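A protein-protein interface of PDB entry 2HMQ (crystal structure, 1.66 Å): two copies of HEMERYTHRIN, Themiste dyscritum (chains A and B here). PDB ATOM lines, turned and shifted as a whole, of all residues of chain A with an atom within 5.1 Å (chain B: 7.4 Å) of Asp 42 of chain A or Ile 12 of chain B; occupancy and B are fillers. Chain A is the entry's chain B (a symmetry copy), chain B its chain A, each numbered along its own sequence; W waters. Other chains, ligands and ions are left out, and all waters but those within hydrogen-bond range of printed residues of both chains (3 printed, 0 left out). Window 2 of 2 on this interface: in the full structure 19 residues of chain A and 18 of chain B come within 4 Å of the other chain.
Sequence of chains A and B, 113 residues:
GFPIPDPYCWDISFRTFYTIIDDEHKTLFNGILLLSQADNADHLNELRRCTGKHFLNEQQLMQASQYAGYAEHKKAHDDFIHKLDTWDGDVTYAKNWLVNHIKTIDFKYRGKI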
ATOM      1  N   LEU A  34      11.503  25.484  24.749  1.00  0.00           N
ATOM      2  CA  LEU A  34      11.854  24.482  23.748  1.00  0.00           C
ATOM      3  C   LEU A  34      11.485  23.063  24.171  1.00  0.00           C
ATOM      4  O   LEU A  34      11.050  22.324  23.285  1.00  0.00           O
ATOM      5  CB  LEU A  34      13.347  24.543  23.410  1.00  0.00           C
ATOM      6  CG  LEU A  34      13.822  25.925  22.941  1.00  0.00           C
ATOM      7  CD1 LEU A  34      15.342  25.837  22.791  1.00  0.00           C
ATOM      8  CD2 LEU A  34      13.098  26.309  21.705  1.00  0.00           C
ATOM      9  N   ASN A  40      13.688  16.775  23.527  1.00  0.00           N
ATOM     10  CA  ASN A  40      14.828  16.062  22.883  1.00  0.00           C
ATOM     11  C   ASN A  40      16.126  16.543  23.499  1.00  0.00           C
ATOM     12  O   ASN A  40      16.143  17.522  24.289  1.00  0.00           O
ATOM     13  CB  ASN A  40      14.566  16.245  21.403  1.00  0.00           C
ATOM     14  CG  ASN A  40      14.739  17.596  20.829  1.00  0.00           C
ATOM     15  OD1 ASN A  40      14.129  17.967  19.810  1.00  0.00           O
ATOM     16  ND2 ASN A  40      15.612  18.422  21.432  1.00  0.00           N
ATOM     17  N   ALA A  41      17.249  16.000  23.090  1.00  0.00           N
ATOM     18  CA  ALA A  41      18.582  16.358  23.499  1.00  0.00           C
ATOM     19  C   ALA A  41      19.071  17.729  22.992  1.00  0.00           C
ATOM     20  O   ALA A  41      19.836  18.344  23.768  1.00  0.00           O
ATOM     21  CB  ALA A  41      19.609  15.287  23.070  1.00  0.00           C
ATOM     22  N   ASP A  42      18.823  18.219  21.813  1.00  0.00           N
ATOM     23  CA  ASP A  42      19.291  19.526  21.426  1.00  0.00           C
ATOM     24  C   ASP A  42      18.710  20.520  22.449  1.00  0.00           C
ATOM     25  O   ASP A  42      19.438  21.380  22.948  1.00  0.00           O
ATOM     26  CB  ASP A  42      18.930  19.878  20.005  1.00  0.00           C
ATOM     27  CG  ASP A  42      19.888  19.280  19.012  1.00  0.00           C
ATOM     28  OD1 ASP A  42      21.077  19.131  19.295  1.00  0.00           O
ATOM     29  OD2 ASP A  42      19.499  18.861  17.903  1.00  0.00           O
ATOM     30  N   HIS A  43      17.437  20.396  22.680  1.00  0.00           N
ATOM     31  CA  HIS A  43      16.758  21.301  23.621  1.00  0.00           C
ATOM     32  C   HIS A  43      17.199  21.173  25.037  1.00  0.00           C
ATOM     33  O   HIS A  43      17.317  22.164  25.789  1.00  0.00           O
ATOM     34  CB  HIS A  43      15.237  21.097  23.525  1.00  0.00           C
ATOM     35  CG  HIS A  43      14.757  21.537  22.169  1.00  0.00           C
ATOM     36  ND1 HIS A  43      13.424  21.270  21.805  1.00  0.00           N
ATOM     37  CD2 HIS A  43      15.276  22.180  21.139  1.00  0.00           C
ATOM     38  CE1 HIS A  43      13.206  21.818  20.617  1.00  0.00           C
ATOM     39  NE2 HIS A  43      14.303  22.359  20.192  1.00  0.00           N
ATOM     40  N   LEU A  44      17.468  19.967  25.521  1.00  0.00           N
ATOM     41  CA  LEU A  44      17.940  19.872  26.904  1.00  0.00           C
ATOM     42  C   LEU A  44      19.377  20.397  27.029  1.00  0.00           C
ATOM     43  O   LEU A  44      19.651  20.925  28.104  1.00  0.00           O
ATOM     44  CB  LEU A  44      17.759  18.464  27.393  1.00  0.00           C
ATOM     45  CG  LEU A  44      18.290  18.110  28.764  1.00  0.00           C
ATOM     46  CD1 LEU A  44      17.450  18.789  29.835  1.00  0.00           C
ATOM     47  CD2 LEU A  44      18.261  16.587  28.922  1.00  0.00           C
ATOM     48  N   ASN A  45      20.189  20.292  26.034  1.00  0.00           N
ATOM     49  CA  ASN A  45      21.607  20.731  26.076  1.00  0.00           C
ATOM     50  C   ASN A  45      21.620  22.273  26.190  1.00  0.00           C
ATOM     51  O   ASN A  45      22.457  22.811  26.893  1.00  0.00           O
ATOM     52  CB  ASN A  45      22.289  20.304  24.842  1.00  0.00           C
ATOM     53  CG  ASN A  45      22.672  18.846  24.760  1.00  0.00           C
ATOM     54  OD1 ASN A  45      23.013  18.401  23.611  1.00  0.00           O
ATOM     55  ND2 ASN A  45      22.628  18.134  25.831  1.00  0.00           N
ATOM     56  N   GLU A  46      20.737  22.817  25.399  1.00  0.00           N
ATOM     57  CA  GLU A  46      20.524  24.269  25.337  1.00  0.00           C
ATOM     58  C   GLU A  46      20.092  24.772  26.667  1.00  0.00           C
ATOM     59  O   GLU A  46      20.778  25.691  27.195  1.00  0.00           O
ATOM     60  CB  GLU A  46      19.515  24.696  24.312  1.00  0.00           C
ATOM     61  CG  GLU A  46      19.604  26.142  23.896  1.00  0.00           C
ATOM     62  CD  GLU A  46      20.844  26.534  23.125  1.00  0.00           C
ATOM     63  OE1 GLU A  46      21.158  27.710  23.078  1.00  0.00           O
ATOM     64  OE2 GLU A  46      21.449  25.639  22.488  1.00  0.00           O
ATOM     65  N   CYS B   9       9.519  33.283  19.547  1.00  0.00           N
ATOM     66  CA  CYS B   9      10.667  32.990  20.372  1.00  0.00           C
ATOM     67  C   CYS B   9      11.697  32.263  19.468  1.00  0.00           C
ATOM     68  O   CYS B   9      11.475  31.756  18.345  1.00  0.00           O
ATOM     69  CB  CYS B   9      10.313  32.259  21.627  1.00  0.00           C
ATOM     70  SG  CYS B   9      10.063  33.368  23.109  1.00  0.00           S
ATOM     71  N   TRP B  10      12.930  32.383  19.984  1.00  0.00           N
ATOM     72  CA  TRP B  10      14.073  31.764  19.317  1.00  0.00           C
ATOM     73  C   TRP B  10      13.910  30.280  19.246  1.00  0.00           C
ATOM     74  O   TRP B  10      13.442  29.652  20.239  1.00  0.00           O
ATOM     75  CB  TRP B  10      15.332  32.195  20.148  1.00  0.00           C
ATOM     76  CG  TRP B  10      16.668  31.733  19.644  1.00  0.00           C
ATOM     77  CD1 TRP B  10      17.546  32.466  18.909  1.00  0.00           C
ATOM     78  CD2 TRP B  10      17.288  30.476  19.884  1.00  0.00           C
ATOM     79  NE1 TRP B  10      18.683  31.729  18.675  1.00  0.00           N
ATOM     80  CE2 TRP B  10      18.577  30.515  19.278  1.00  0.00           C
ATOM     81  CE3 TRP B  10      16.940  29.338  20.621  1.00  0.00           C
ATOM     82  CZ2 TRP B  10      19.455  29.462  19.337  1.00  0.00           C
ATOM     83  CZ3 TRP B  10      17.780  28.300  20.657  1.00  0.00           C
ATOM     84  CH2 TRP B  10      19.061  28.342  20.061  1.00  0.00           C
ATOM     85  N   ASP B  11      14.393  29.602  18.240  1.00  0.00           N
ATOM     86  CA  ASP B  11      14.391  28.104  18.233  1.00  0.00           C
ATOM     87  C   ASP B  11      15.766  27.680  17.732  1.00  0.00           C
ATOM     88  O   ASP B  11      16.456  28.586  17.203  1.00  0.00           O
ATOM     89  CB  ASP B  11      13.190  27.561  17.488  1.00  0.00           C
ATOM     90  CG  ASP B  11      13.198  27.882  16.009  1.00  0.00           C
ATOM     91  OD1 ASP B  11      14.160  27.498  15.293  1.00  0.00           O
ATOM     92  OD2 ASP B  11      12.241  28.485  15.507  1.00  0.00           O
ATOM     93  N   ILE B  12      16.094  26.408  17.812  1.00  0.00           N
ATOM     94  CA  ILE B  12      17.453  25.999  17.385  1.00  0.00           C
ATOM     95  C   ILE B  12      17.742  26.155  15.918  1.00  0.00           C
ATOM     96  O   ILE B  12      18.968  26.124  15.549  1.00  0.00           O
ATOM     97  CB  ILE B  12      17.850  24.577  17.952  1.00  0.00           C
ATOM     98  CG1 ILE B  12      17.087  23.544  17.111  1.00  0.00           C
ATOM     99  CG2 ILE B  12      17.694  24.501  19.483  1.00  0.00           C
ATOM    100  CD1 ILE B  12      17.006  22.114  17.684  1.00  0.00           C
ATOM    101  N   SER B  13      16.816  26.413  15.031  1.00  0.00           N
ATOM    102  CA  SER B  13      17.078  26.692  13.632  1.00  0.00           C
ATOM    103  C   SER B  13      17.878  27.987  13.451  1.00  0.00           C
ATOM    104  O   SER B  13      18.404  28.275  12.384  1.00  0.00           O
ATOM    105  CB  SER B  13      15.788  26.712  12.812  1.00  0.00           C
ATOM    106  OG  SER B  13      15.077  27.892  12.768  1.00  0.00           O
ATOM    107  N   PHE B  14      17.876  28.848  14.477  1.00  0.00           N
ATOM    108  CA  PHE B  14      18.549  30.149  14.461  1.00  0.00           C
ATOM    109  C   PHE B  14      19.954  29.994  14.970  1.00  0.00           C
ATOM    110  O   PHE B  14      20.629  31.008  15.016  1.00  0.00           O
ATOM    111  CB  PHE B  14      17.715  31.152  15.306  1.00  0.00           C
ATOM    112  CG  PHE B  14      16.523  31.620  14.523  1.00  0.00           C
ATOM    113  CD1 PHE B  14      15.301  30.951  14.708  1.00  0.00           C
ATOM    114  CD2 PHE B  14      16.583  32.619  13.598  1.00  0.00           C
ATOM    115  CE1 PHE B  14      14.213  31.332  13.954  1.00  0.00           C
ATOM    116  CE2 PHE B  14      15.514  33.063  12.868  1.00  0.00           C
ATOM    117  CZ  PHE B  14      14.260  32.407  13.056  1.00  0.00           C
ATOM    118  N   ARG B  15      20.334  28.795  15.342  1.00  0.00           N
ATOM    119  CA  ARG B  15      21.696  28.655  15.902  1.00  0.00           C
ATOM    120  C   ARG B  15      22.780  29.160  14.959  1.00  0.00           C
ATOM    121  O   ARG B  15      22.817  28.734  13.847  1.00  0.00           O
ATOM    122  CB  ARG B  15      22.090  27.281  16.257  1.00  0.00           C
ATOM    123  CG  ARG B  15      21.735  26.802  17.577  1.00  0.00           C
ATOM    124  CD  ARG B  15      22.157  25.426  17.829  1.00  0.00           C
ATOM    125  NE  ARG B  15      21.567  24.960  19.075  1.00  0.00           N
ATOM    126  CZ  ARG B  15      21.265  23.674  19.316  1.00  0.00           C
ATOM    127  NH1 ARG B  15      21.406  22.770  18.314  1.00  0.00           N
ATOM    128  NH2 ARG B  15      21.220  23.298  20.634  1.00  0.00           N
ATOM    129  N   THR B  16      23.718  29.968  15.504  1.00  0.00           N
ATOM    130  CA  THR B  16      24.833  30.446  14.718  1.00  0.00           C
ATOM    131  C   THR B  16      26.068  29.633  15.034  1.00  0.00           C
ATOM    132  O   THR B  16      27.089  29.652  14.343  1.00  0.00           O
ATOM    133  CB  THR B  16      25.146  31.983  14.944  1.00  0.00           C
ATOM    134  OG1 THR B  16      25.587  32.015  16.337  1.00  0.00           O
ATOM    135  CG2 THR B  16      24.027  32.900  14.562  1.00  0.00           C
ATOM    136  N   PHE B  17      26.043  28.912  16.124  1.00  0.00           N
ATOM    137  CA  PHE B  17      27.183  28.176  16.645  1.00  0.00           C
ATOM    138  C   PHE B  17      28.128  28.982  17.501  1.00  0.00           C
ATOM    139  O   PHE B  17      29.074  28.431  18.046  1.00  0.00           O
ATOM    140  CB  PHE B  17      27.940  27.372  15.519  1.00  0.00           C
ATOM    141  CG  PHE B  17      26.932  26.264  15.181  1.00  0.00           C
ATOM    142  CD1 PHE B  17      26.518  25.351  16.182  1.00  0.00           C
ATOM    143  CD2 PHE B  17      26.305  26.279  13.946  1.00  0.00           C
ATOM    144  CE1 PHE B  17      25.525  24.428  15.961  1.00  0.00           C
ATOM    145  CE2 PHE B  17      25.296  25.318  13.692  1.00  0.00           C
ATOM    146  CZ  PHE B  17      24.897  24.421  14.712  1.00  0.00           C
ATOM    147  N   ASP B  22      24.109  33.498  20.144  1.00  0.00           N
ATOM    148  CA  ASP B  22      22.781  32.850  20.236  1.00  0.00           C
ATOM    149  C   ASP B  22      22.056  33.360  21.499  1.00  0.00           C
ATOM    150  O   ASP B  22      20.859  33.615  21.390  1.00  0.00           O
ATOM    151  CB  ASP B  22      22.863  31.300  20.249  1.00  0.00           C
ATOM    152  CG  ASP B  22      23.359  30.774  18.879  1.00  0.00           C
ATOM    153  OD1 ASP B  22      23.297  31.438  17.858  1.00  0.00           O
ATOM    154  OD2 ASP B  22      23.762  29.609  18.987  1.00  0.00           O
ATOM    155  N   LYS B  26      18.345  35.436  21.624  1.00  0.00           N
ATOM    156  CA  LYS B  26      17.156  35.043  22.398  1.00  0.00           C
ATOM    157  C   LYS B  26      16.534  36.259  23.023  1.00  0.00           C
ATOM    158  O   LYS B  26      15.310  36.359  23.132  1.00  0.00           O
ATOM    159  CB  LYS B  26      17.541  33.989  23.420  1.00  0.00           C
ATOM    160  CG  LYS B  26      17.991  32.635  22.890  1.00  0.00           C
ATOM    161  CD  LYS B  26      18.601  31.713  23.901  1.00  0.00           C
ATOM    162  CE  LYS B  26      19.337  30.560  23.283  1.00  0.00           C
ATOM    163  NZ  LYS B  26      20.029  29.728  24.246  1.00  0.00           N
ATOM    164  N   LYS B 103      19.152  34.710   9.770  1.00  0.00           N
ATOM    165  CA  LYS B 103      19.293  33.621   8.764  1.00  0.00           C
ATOM    166  C   LYS B 103      19.972  34.020   7.526  1.00  0.00           C
ATOM    167  O   LYS B 103      20.586  33.144   6.819  1.00  0.00           O
ATOM    168  CB  LYS B 103      17.881  32.996   8.555  1.00  0.00           C
ATOM    169  CG  LYS B 103      17.664  32.029   9.744  1.00  0.00           C
ATOM    170  CD  LYS B 103      16.301  31.332   9.591  1.00  0.00           C
ATOM    171  CE  LYS B 103      16.259  30.156  10.581  1.00  0.00           C
ATOM    172  NZ  LYS B 103      14.837  29.620  10.531  1.00  0.00           N
ATOM    173  N   PHE B 107      24.173  34.665   9.462  1.00  0.00           N
ATOM    174  CA  PHE B 107      24.662  33.340   9.049  1.00  0.00           C
ATOM    175  C   PHE B 107      25.853  33.482   8.117  1.00  0.00           C
ATOM    176  O   PHE B 107      26.656  32.537   8.104  1.00  0.00           O
ATOM    177  CB  PHE B 107      23.555  32.445   8.435  1.00  0.00           C
ATOM    178  CG  PHE B 107      22.740  31.671   9.413  1.00  0.00           C
ATOM    179  CD1 PHE B 107      21.897  30.623   8.906  1.00  0.00           C
ATOM    180  CD2 PHE B 107      22.627  31.978  10.764  1.00  0.00           C
ATOM    181  CE1 PHE B 107      21.082  29.929   9.747  1.00  0.00           C
ATOM    182  CE2 PHE B 107      21.863  31.211  11.627  1.00  0.00           C
ATOM    183  CZ  PHE B 107      21.053  30.202  11.088  1.00  0.00           C
HETATM  184  O   HOH W   1      22.485  20.975  21.731  1.00  0.00           O
HETATM  185  O   HOH W   2      23.220  27.573  20.690  1.00  0.00           O
HETATM  186  O   HOH W   3      13.808  24.274  18.294  1.00  0.00           O
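OD1 of Asp 42 of chain A is in salt-bridge range of NH1 of Arg 15 of chain B, at 3.8 Å. The guanidinium group (NH2) of Arg 15 of chain B is in salt-bridge range of the side-chain carboxylate (OE2) of Glu 46 of chain A, at 3.0 Å. The side-chain amino group (NZ) of Lys 26 of chain B is in salt-bridge range of the side-chain carboxylate (OE1) of Glu 46 of chain A, 2.6 Å away.
The backbone carbonyl oxygen of Leu 34 of chain A is in hydrogen-bond range of a ring nitrogen (ND1) of His 43 of chain A. ND2 of Asn 40 of chain A sits close to N of Asp 42 of chain A. The side-chain amide nitrogen (ND2) of Asn 40 of chain A lies close to the backbone NH (N) of His 43 of chain A, at 3.0 Å.
Among the printed residues, pairs that only touch across the chains: Leu 34 of chain A with Trp 10 of chain B (3.7 Å), Asp 42 of chain A with Ile 12 of chain B (3.8 Å), His 43 of chain A with Ile 12 of chain B (3.7 Å) and Glu 46 of chain A with Trp 10 of chain B (3.7 Å).
Of chain B, only Ile 12 and Arg 15 come within 4 Å of Asp 42 of chain A. Printed residues of chain A within 4 Å of Ile 12 of chain B: Asp 42 (3.8 Å) and His 43 (3.7 Å). No residue of chain B comes within 4 Å of Ala 41 of chain A. Of the printed residues of chain A, Arg 15 of chain B touches Asp 42 and Glu 46. Of the printed residues of chain A, Trp 10 of chain B touches Leu 34 (3.7 Å) and Glu 46 (3.7 Å). Phe 107 of chain B touches none of the printed residues of chain A. Phe 14 of chain B touches none of the printed residues of chain A.
Of the 8 printed residues of chain A, 4 touch a printed residue of chain B. Along chain A the printed residues that touch a printed residue of chain B span positions 34 to 46. Among the printed residues, 7 pairs touch across the chains.
No position is printed for both chains. Of the 7 pairs that touch across the chains among the printed residues, none has its exchanged pair printed and touching as well.
Water W2 lies within hydrogen-bond range of the side-chain carboxylate (OD2) of Asp 22 of chain B, the side-chain carboxylate (OE1) of Glu 46 of chain A and the guanidinium group (NE) of Arg 15 of chain B. Water W3 bridges NE2 of His 43 of chain A (2.7 Å) and N of Ile 12 of chain B (3.2 Å). Water W1 lies within hydrogen-bond range of the guanidinium group of Arg 15 of chain B (2.9 Å), the side-chain amide oxygen of Asn 45 of chain A (3.2 Å) and the backbone carbonyl oxygen of Asp 42 of chain A (3.3 Å).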
